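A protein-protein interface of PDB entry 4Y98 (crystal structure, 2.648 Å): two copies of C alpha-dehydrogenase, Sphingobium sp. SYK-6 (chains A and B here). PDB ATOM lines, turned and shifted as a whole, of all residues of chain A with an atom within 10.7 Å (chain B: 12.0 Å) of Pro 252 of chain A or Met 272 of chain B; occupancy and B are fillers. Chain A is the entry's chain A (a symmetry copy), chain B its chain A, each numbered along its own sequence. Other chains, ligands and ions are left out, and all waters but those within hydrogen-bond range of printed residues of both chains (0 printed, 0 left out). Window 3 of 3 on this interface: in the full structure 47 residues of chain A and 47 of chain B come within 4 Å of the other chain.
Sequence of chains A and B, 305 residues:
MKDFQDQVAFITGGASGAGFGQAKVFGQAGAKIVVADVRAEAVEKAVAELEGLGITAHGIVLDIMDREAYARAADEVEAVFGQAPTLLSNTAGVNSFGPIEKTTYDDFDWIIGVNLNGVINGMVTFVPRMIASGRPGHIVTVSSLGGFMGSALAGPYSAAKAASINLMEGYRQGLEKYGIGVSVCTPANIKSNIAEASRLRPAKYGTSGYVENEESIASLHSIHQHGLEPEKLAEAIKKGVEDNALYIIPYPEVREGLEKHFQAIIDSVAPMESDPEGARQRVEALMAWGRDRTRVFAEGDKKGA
Ile 249 of chain A touches Ile 265 of chain B. O of Ile 249 of chain A touches CA of Val 269 of chain B, at 3.7 Å. Pro 250 of chain A touches Ala 270 of chain B (CA to CB, 3.8 Å). CG1 of Val 269 of chain B touches O of Tyr 251 of chain A (3.9 Å). CG1 of Val 269 of chain B touches CA of Pro 252 of chain A, at 3.9 Å. Pro 252 of chain A touches Ala 270 of chain B. CB of Pro 252 of chain A touches C of Met 272 of chain B (3.3 Å). O of Val 269 of chain B touches NH1 of Arg 255 of chain A, at 3.7 Å. Ile 266 of chain B touches Glu 259 of chain A.
No position is printed for both chains. Of the 12 pairs that touch across the chains among the printed residues, none has its exchanged pair printed and touching as well.
NH1 of Arg 255 of chain A lies within hydrogen-bond range of O of Ile 266 of chain B (3.4 Å). The side-chain carboxylate (OD1) of Asp 267 of chain B lies within salt-bridge range of the guanidinium group (NH2) of Arg 255 of chain A, 3.8 Å away. The backbone NH (N) of Ala 270 of chain B sits at hydrogen-bond distance from the backbone carbonyl oxygen (O) of Ile 249 of chain A (3.1 Å).
Gly 227 of chain A touches none of the printed residues of chain B. Of the printed residues of chain B, Pro 252 of chain A touches Val 269, Ala 270 and Met 272. No residue of chain B comes within 4 Å of Glu 253 of chain A. No residue of chain B comes within 4 Å of Val 254 of chain A. Of the printed residues of chain B, Glu 259 of chain A touches Ile 266. Of the printed residues of chain A, Asp 267 of chain B touches Arg 255. Ser 268 of chain B touches none of the printed residues of chain A. Of the printed residues of chain A, Ala 270 of chain B touches Ile 249, Pro 250 and Pro 252. Of chain A, only Pro 252 comes within 4 Å of Met 272 of chain B. The nearest printed residue of chain B that does not touch Pro 252 of chain A is Pro 271 of chain B (4.02 Å). The nearest residue of chain A that does not touch Met 272 of chain B is Glu 253 of chain A (6.0 Å).
Hydrophobic or aromatic side chains of chain A that line the printed part of chain B: Ile 249 and Pro 252. Among the printed residues, 12 pairs touch across the chains.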
ATOM      1  N   LEU A 145      -4.594  23.901  -6.987  1.00  0.00           N
ATOM      2  CA  LEU A 145      -3.835  23.708  -8.215  1.00  0.00           C
ATOM      3  C   LEU A 145      -4.090  24.867  -9.170  1.00  0.00           C
ATOM      4  O   LEU A 145      -3.248  25.198 -10.007  1.00  0.00           O
ATOM      5  CB  LEU A 145      -4.227  22.388  -8.865  1.00  0.00           C
ATOM      6  CG  LEU A 145      -3.335  21.884  -9.992  1.00  0.00           C
ATOM      7  CD1 LEU A 145      -2.064  21.284  -9.409  1.00  0.00           C
ATOM      8  CD2 LEU A 145      -4.088  20.866 -10.844  1.00  0.00           C
ATOM      9  N   THR A 186      -1.908  21.874  -2.658  1.00  0.00           N
ATOM     10  CA  THR A 186      -2.584  22.374  -3.852  1.00  0.00           C
ATOM     11  C   THR A 186      -3.446  21.270  -4.422  1.00  0.00           C
ATOM     12  O   THR A 186      -3.026  20.545  -5.319  1.00  0.00           O
ATOM     13  CB  THR A 186      -1.581  22.890  -4.930  1.00  0.00           C
ATOM     14  OG1 THR A 186      -0.854  21.794  -5.499  1.00  0.00           O
ATOM     15  CG2 THR A 186      -0.610  23.891  -4.320  1.00  0.00           C
ATOM     16  N   PRO A 187      -4.658  21.123  -3.883  1.00  0.00           N
ATOM     17  CA  PRO A 187      -5.557  20.099  -4.414  1.00  0.00           C
ATOM     18  C   PRO A 187      -6.001  20.406  -5.842  1.00  0.00           C
ATOM     19  O   PRO A 187      -5.959  21.565  -6.257  1.00  0.00           O
ATOM     20  CB  PRO A 187      -6.747  20.141  -3.448  1.00  0.00           C
ATOM     21  CG  PRO A 187      -6.234  20.819  -2.225  1.00  0.00           C
ATOM     22  CD  PRO A 187      -5.218  21.786  -2.692  1.00  0.00           C
ATOM     23  N   ALA A 188      -6.425  19.371  -6.567  1.00  0.00           N
ATOM     24  CA  ALA A 188      -6.903  19.510  -7.938  1.00  0.00           C
ATOM     25  C   ALA A 188      -8.412  19.702  -8.012  1.00  0.00           C
ATOM     26  O   ALA A 188      -9.141  18.769  -8.336  1.00  0.00           O
ATOM     27  CB  ALA A 188      -6.503  18.298  -8.747  1.00  0.00           C
ATOM     28  N   GLY A 227     -12.263  12.437  -7.591  1.00  0.00           N
ATOM     29  CA  GLY A 227     -11.712  13.475  -6.738  1.00  0.00           C
ATOM     30  C   GLY A 227     -11.248  12.852  -5.436  1.00  0.00           C
ATOM     31  O   GLY A 227     -11.868  11.911  -4.943  1.00  0.00           O
ATOM     32  N   LEU A 228     -10.157  13.366  -4.878  1.00  0.00           N
ATOM     33  CA  LEU A 228      -9.546  12.748  -3.706  1.00  0.00           C
ATOM     34  C   LEU A 228     -10.358  13.036  -2.437  1.00  0.00           C
ATOM     35  O   LEU A 228     -10.710  14.182  -2.159  1.00  0.00           O
ATOM     36  CB  LEU A 228      -8.102  13.236  -3.545  1.00  0.00           C
ATOM     37  CG  LEU A 228      -7.095  12.184  -3.065  1.00  0.00           C
ATOM     38  CD1 LEU A 228      -6.790  11.169  -4.164  1.00  0.00           C
ATOM     39  CD2 LEU A 228      -5.812  12.831  -2.579  1.00  0.00           C
ATOM     40  N   LEU A 233      -6.823  13.130   1.436  1.00  0.00           N
ATOM     41  CA  LEU A 233      -6.056  14.372   1.338  1.00  0.00           C
ATOM     42  C   LEU A 233      -5.480  14.787   2.683  1.00  0.00           C
ATOM     43  O   LEU A 233      -4.396  15.367   2.752  1.00  0.00           O
ATOM     44  CB  LEU A 233      -6.930  15.499   0.787  1.00  0.00           C
ATOM     45  CG  LEU A 233      -6.257  16.878   0.696  1.00  0.00           C
ATOM     46  CD1 LEU A 233      -5.055  16.847  -0.239  1.00  0.00           C
ATOM     47  CD2 LEU A 233      -7.237  17.959   0.252  1.00  0.00           C
ATOM     48  N   ALA A 236      -2.398  13.002   3.378  1.00  0.00           N
ATOM     49  CA  ALA A 236      -1.344  13.544   2.515  1.00  0.00           C
ATOM     50  C   ALA A 236      -0.719  14.783   3.128  1.00  0.00           C
ATOM     51  O   ALA A 236       0.483  14.999   3.022  1.00  0.00           O
ATOM     52  CB  ALA A 236      -1.891  13.870   1.142  1.00  0.00           C
ATOM     53  N   ILE A 248       2.632  20.018  -1.423  1.00  0.00           N
ATOM     54  CA  ILE A 248       1.889  18.795  -1.203  1.00  0.00           C
ATOM     55  C   ILE A 248       0.887  18.630  -2.332  1.00  0.00           C
ATOM     56  O   ILE A 248      -0.195  19.213  -2.313  1.00  0.00           O
ATOM     57  CB  ILE A 248       1.182  18.805   0.155  1.00  0.00           C
ATOM     58  CG1 ILE A 248       2.179  19.212   1.241  1.00  0.00           C
ATOM     59  CG2 ILE A 248       0.641  17.428   0.446  1.00  0.00           C
ATOM     60  CD1 ILE A 248       1.620  19.237   2.640  1.00  0.00           C
ATOM     61  N   ILE A 249       1.270  17.831  -3.319  1.00  0.00           N
ATOM     62  CA  ILE A 249       0.485  17.669  -4.532  1.00  0.00           C
ATOM     63  C   ILE A 249       0.189  16.192  -4.784  1.00  0.00           C
ATOM     64  O   ILE A 249       0.789  15.566  -5.652  1.00  0.00           O
ATOM     65  CB  ILE A 249       1.209  18.257  -5.755  1.00  0.00           C
ATOM     66  CG1 ILE A 249       1.827  19.624  -5.409  1.00  0.00           C
ATOM     67  CG2 ILE A 249       0.226  18.367  -6.904  1.00  0.00           C
ATOM     68  CD1 ILE A 249       2.688  20.251  -6.532  1.00  0.00           C
ATOM     69  N   PRO A 250      -0.748  15.628  -4.014  1.00  0.00           N
ATOM     70  CA  PRO A 250      -1.006  14.187  -4.050  1.00  0.00           C
ATOM     71  C   PRO A 250      -1.896  13.774  -5.222  1.00  0.00           C
ATOM     72  O   PRO A 250      -2.880  13.059  -5.039  1.00  0.00           O
ATOM     73  CB  PRO A 250      -1.685  13.946  -2.710  1.00  0.00           C
ATOM     74  CG  PRO A 250      -2.396  15.226  -2.413  1.00  0.00           C
ATOM     75  CD  PRO A 250      -1.548  16.308  -2.978  1.00  0.00           C
ATOM     76  N   TYR A 251      -1.543  14.238  -6.420  1.00  0.00           N
ATOM     77  CA  TYR A 251      -2.350  13.994  -7.608  1.00  0.00           C
ATOM     78  C   TYR A 251      -1.502  13.684  -8.836  1.00  0.00           C
ATOM     79  O   TYR A 251      -1.461  14.480  -9.763  1.00  0.00           O
ATOM     80  CB  TYR A 251      -3.231  15.204  -7.898  1.00  0.00           C
ATOM     81  CG  TYR A 251      -4.161  15.560  -6.770  1.00  0.00           C
ATOM     82  CD1 TYR A 251      -3.732  16.350  -5.712  1.00  0.00           C
ATOM     83  CD2 TYR A 251      -5.473  15.101  -6.760  1.00  0.00           C
ATOM     84  CE1 TYR A 251      -4.584  16.669  -4.676  1.00  0.00           C
ATOM     85  CE2 TYR A 251      -6.333  15.420  -5.731  1.00  0.00           C
ATOM     86  CZ  TYR A 251      -5.885  16.203  -4.694  1.00  0.00           C
ATOM     87  OH  TYR A 251      -6.738  16.519  -3.666  1.00  0.00           O
ATOM     88  N   PRO A 252      -0.865  12.500  -8.865  1.00  0.00           N
ATOM     89  CA  PRO A 252       0.040  12.099  -9.954  1.00  0.00           C
ATOM     90  C   PRO A 252      -0.433  12.458 -11.366  1.00  0.00           C
ATOM     91  O   PRO A 252       0.392  12.593 -12.274  1.00  0.00           O
ATOM     92  CB  PRO A 252       0.119  10.570  -9.806  1.00  0.00           C
ATOM     93  CG  PRO A 252      -0.918  10.194  -8.794  1.00  0.00           C
ATOM     94  CD  PRO A 252      -1.111  11.389  -7.933  1.00  0.00           C
ATOM     95  N   GLU A 253      -1.738  12.626 -11.543  1.00  0.00           N
ATOM     96  CA  GLU A 253      -2.303  12.878 -12.862  1.00  0.00           C
ATOM     97  C   GLU A 253      -1.984  14.267 -13.411  1.00  0.00           C
ATOM     98  O   GLU A 253      -1.850  14.432 -14.621  1.00  0.00           O
ATOM     99  CB  GLU A 253      -3.823  12.684 -12.841  1.00  0.00           C
ATOM    100  CG  GLU A 253      -4.545  13.382 -11.693  1.00  0.00           C
ATOM    101  CD  GLU A 253      -4.625  12.541 -10.423  1.00  0.00           C
ATOM    102  OE1 GLU A 253      -5.172  13.041  -9.420  1.00  0.00           O
ATOM    103  OE2 GLU A 253      -4.140  11.391 -10.417  1.00  0.00           O
ATOM    104  N   VAL A 254      -1.854  15.262 -12.538  1.00  0.00           N
ATOM    105  CA  VAL A 254      -1.673  16.645 -12.986  1.00  0.00           C
ATOM    106  C   VAL A 254      -0.285  16.957 -13.548  1.00  0.00           C
ATOM    107  O   VAL A 254      -0.084  18.012 -14.151  1.00  0.00           O
ATOM    108  CB  VAL A 254      -1.930  17.641 -11.843  1.00  0.00           C
ATOM    109  CG1 VAL A 254      -3.306  17.422 -11.255  1.00  0.00           C
ATOM    110  CG2 VAL A 254      -0.854  17.519 -10.770  1.00  0.00           C
ATOM    111  N   ARG A 255       0.663  16.051 -13.339  1.00  0.00           N
ATOM    112  CA  ARG A 255       2.058  16.311 -13.666  1.00  0.00           C
ATOM    113  C   ARG A 255       2.233  16.809 -15.103  1.00  0.00           C
ATOM    114  O   ARG A 255       2.917  17.805 -15.340  1.00  0.00           O
ATOM    115  CB  ARG A 255       2.883  15.049 -13.433  1.00  0.00           C
ATOM    116  CG  ARG A 255       4.374  15.241 -13.544  1.00  0.00           C
ATOM    117  CD  ARG A 255       5.111  14.272 -12.632  1.00  0.00           C
ATOM    118  NE  ARG A 255       6.561  14.401 -12.752  1.00  0.00           N
ATOM    119  CZ  ARG A 255       7.435  14.057 -11.810  1.00  0.00           C
ATOM    120  NH1 ARG A 255       7.021  13.560 -10.649  1.00  0.00           N
ATOM    121  NH2 ARG A 255       8.735  14.220 -12.031  1.00  0.00           N
ATOM    122  N   GLU A 256       1.584  16.140 -16.050  1.00  0.00           N
ATOM    123  CA  GLU A 256       1.728  16.482 -17.462  1.00  0.00           C
ATOM    124  C   GLU A 256       1.336  17.940 -17.722  1.00  0.00           C
ATOM    125  O   GLU A 256       2.089  18.697 -18.336  1.00  0.00           O
ATOM    126  CB  GLU A 256       0.881  15.540 -18.325  1.00  0.00           C
ATOM    127  CG  GLU A 256       1.344  15.423 -19.774  1.00  0.00           C
ATOM    128  CD  GLU A 256       0.571  14.377 -20.562  1.00  0.00           C
ATOM    129  OE1 GLU A 256      -0.469  13.894 -20.064  1.00  0.00           O
ATOM    130  OE2 GLU A 256       1.007  14.034 -21.683  1.00  0.00           O
ATOM    131  N   GLY A 257       0.167  18.332 -17.230  1.00  0.00           N
ATOM    132  CA  GLY A 257      -0.376  19.654 -17.490  1.00  0.00           C
ATOM    133  C   GLY A 257       0.421  20.756 -16.821  1.00  0.00           C
ATOM    134  O   GLY A 257       0.536  21.871 -17.338  1.00  0.00           O
ATOM    135  N   LEU A 258       0.961  20.440 -15.653  1.00  0.00           N
ATOM    136  CA  LEU A 258       1.747  21.390 -14.890  1.00  0.00           C
ATOM    137  C   LEU A 258       3.071  21.630 -15.598  1.00  0.00           C
ATOM    138  O   LEU A 258       3.562  22.756 -15.659  1.00  0.00           O
ATOM    139  CB  LEU A 258       1.973  20.867 -13.477  1.00  0.00           C
ATOM    140  CG  LEU A 258       1.590  21.744 -12.282  1.00  0.00           C
ATOM    141  CD1 LEU A 258       0.263  22.467 -12.467  1.00  0.00           C
ATOM    142  CD2 LEU A 258       1.529  20.856 -11.046  1.00  0.00           C
ATOM    143  N   GLU A 259       3.649  20.559 -16.128  1.00  0.00           N
ATOM    144  CA  GLU A 259       4.863  20.670 -16.917  1.00  0.00           C
ATOM    145  C   GLU A 259       4.606  21.554 -18.135  1.00  0.00           C
ATOM    146  O   GLU A 259       5.438  22.376 -18.510  1.00  0.00           O
ATOM    147  CB  GLU A 259       5.355  19.288 -17.359  1.00  0.00           C
ATOM    148  CG  GLU A 259       5.967  18.438 -16.254  1.00  0.00           C
ATOM    149  CD  GLU A 259       6.317  17.036 -16.727  1.00  0.00           C
ATOM    150  OE1 GLU A 259       5.487  16.414 -17.424  1.00  0.00           O
ATOM    151  OE2 GLU A 259       7.424  16.553 -16.403  1.00  0.00           O
ATOM    152  N   ILE B 265       8.611  22.044  -8.021  1.00  0.00           N
ATOM    153  CA  ILE B 265       7.179  21.817  -7.940  1.00  0.00           C
ATOM    154  C   ILE B 265       6.810  20.487  -8.594  1.00  0.00           C
ATOM    155  O   ILE B 265       6.219  19.629  -7.946  1.00  0.00           O
ATOM    156  CB  ILE B 265       6.394  22.960  -8.592  1.00  0.00           C
ATOM    157  CG1 ILE B 265       6.680  24.266  -7.855  1.00  0.00           C
ATOM    158  CG2 ILE B 265       4.898  22.677  -8.564  1.00  0.00           C
ATOM    159  CD1 ILE B 265       6.373  25.494  -8.671  1.00  0.00           C
ATOM    160  N   ILE B 266       7.165  20.306  -9.860  1.00  0.00           N
ATOM    161  CA  ILE B 266       6.862  19.067 -10.568  1.00  0.00           C
ATOM    162  C   ILE B 266       7.357  17.848  -9.795  1.00  0.00           C
ATOM    163  O   ILE B 266       6.666  16.834  -9.704  1.00  0.00           O
ATOM    164  CB  ILE B 266       7.482  19.067 -11.976  1.00  0.00           C
ATOM    165  CG1 ILE B 266       6.466  19.569 -12.994  1.00  0.00           C
ATOM    166  CG2 ILE B 266       7.931  17.668 -12.384  1.00  0.00           C
ATOM    167  CD1 ILE B 266       5.926  20.927 -12.675  1.00  0.00           C
ATOM    168  N   ASP B 267       8.556  17.949  -9.242  1.00  0.00           N
ATOM    169  CA  ASP B 267       9.130  16.853  -8.482  1.00  0.00           C
ATOM    170  C   ASP B 267       8.315  16.553  -7.226  1.00  0.00           C
ATOM    171  O   ASP B 267       8.348  15.437  -6.720  1.00  0.00           O
ATOM    172  CB  ASP B 267      10.576  17.173  -8.108  1.00  0.00           C
ATOM    173  CG  ASP B 267      11.522  17.040  -9.283  1.00  0.00           C
ATOM    174  OD1 ASP B 267      11.034  16.849 -10.419  1.00  0.00           O
ATOM    175  OD2 ASP B 267      12.753  17.134  -9.073  1.00  0.00           O
ATOM    176  N   SER B 268       7.581  17.542  -6.729  1.00  0.00           N
ATOM    177  CA  SER B 268       6.774  17.345  -5.530  1.00  0.00           C
ATOM    178  C   SER B 268       5.509  16.549  -5.834  1.00  0.00           C
ATOM    179  O   SER B 268       4.872  16.017  -4.924  1.00  0.00           O
ATOM    180  CB  SER B 268       6.389  18.685  -4.901  1.00  0.00           C
ATOM    181  OG  SER B 268       7.494  19.302  -4.264  1.00  0.00           O
ATOM    182  N   VAL B 269       5.141  16.477  -7.108  1.00  0.00           N
ATOM    183  CA  VAL B 269       3.945  15.746  -7.495  1.00  0.00           C
ATOM    184  C   VAL B 269       4.102  14.272  -7.129  1.00  0.00           C
ATOM    185  O   VAL B 269       5.084  13.631  -7.506  1.00  0.00           O
ATOM    186  CB  VAL B 269       3.649  15.884  -8.998  1.00  0.00           C
ATOM    187  CG1 VAL B 269       2.376  15.135  -9.350  1.00  0.00           C
ATOM    188  CG2 VAL B 269       3.511  17.349  -9.381  1.00  0.00           C
ATOM    189  N   ALA B 270       3.131  13.752  -6.382  1.00  0.00           N
ATOM    190  CA  ALA B 270       3.177  12.378  -5.889  1.00  0.00           C
ATOM    191  C   ALA B 270       3.245  11.386  -7.041  1.00  0.00           C
ATOM    192  O   ALA B 270       2.597  11.585  -8.068  1.00  0.00           O
ATOM    193  CB  ALA B 270       1.956  12.080  -5.010  1.00  0.00           C
ATOM    194  N   PRO B 271       4.049  10.322  -6.885  1.00  0.00           N
ATOM    195  CA  PRO B 271       3.868   9.183  -7.786  1.00  0.00           C
ATOM    196  C   PRO B 271       2.568   8.455  -7.428  1.00  0.00           C
ATOM    197  O   PRO B 271       2.058   8.690  -6.333  1.00  0.00           O
ATOM    198  CB  PRO B 271       5.103   8.319  -7.517  1.00  0.00           C
ATOM    199  CG  PRO B 271       5.493   8.654  -6.121  1.00  0.00           C
ATOM    200  CD  PRO B 271       5.151  10.101  -5.931  1.00  0.00           C
ATOM    201  N   MET B 272       2.037   7.602  -8.303  1.00  0.00           N
ATOM    202  CA  MET B 272       2.654   7.260  -9.579  1.00  0.00           C
ATOM    203  C   MET B 272       2.024   8.059 -10.713  1.00  0.00           C
ATOM    204  O   MET B 272       1.531   7.497 -11.690  1.00  0.00           O
ATOM    205  CB  MET B 272       2.519   5.755  -9.842  1.00  0.00           C
ATOM    206  CG  MET B 272       1.086   5.242  -9.814  1.00  0.00           C
ATOM    207  SD  MET B 272       0.841   3.888  -8.644  1.00  0.00           S
ATOM    208  CE  MET B 272       1.200   4.716  -7.096  1.00  0.00           C
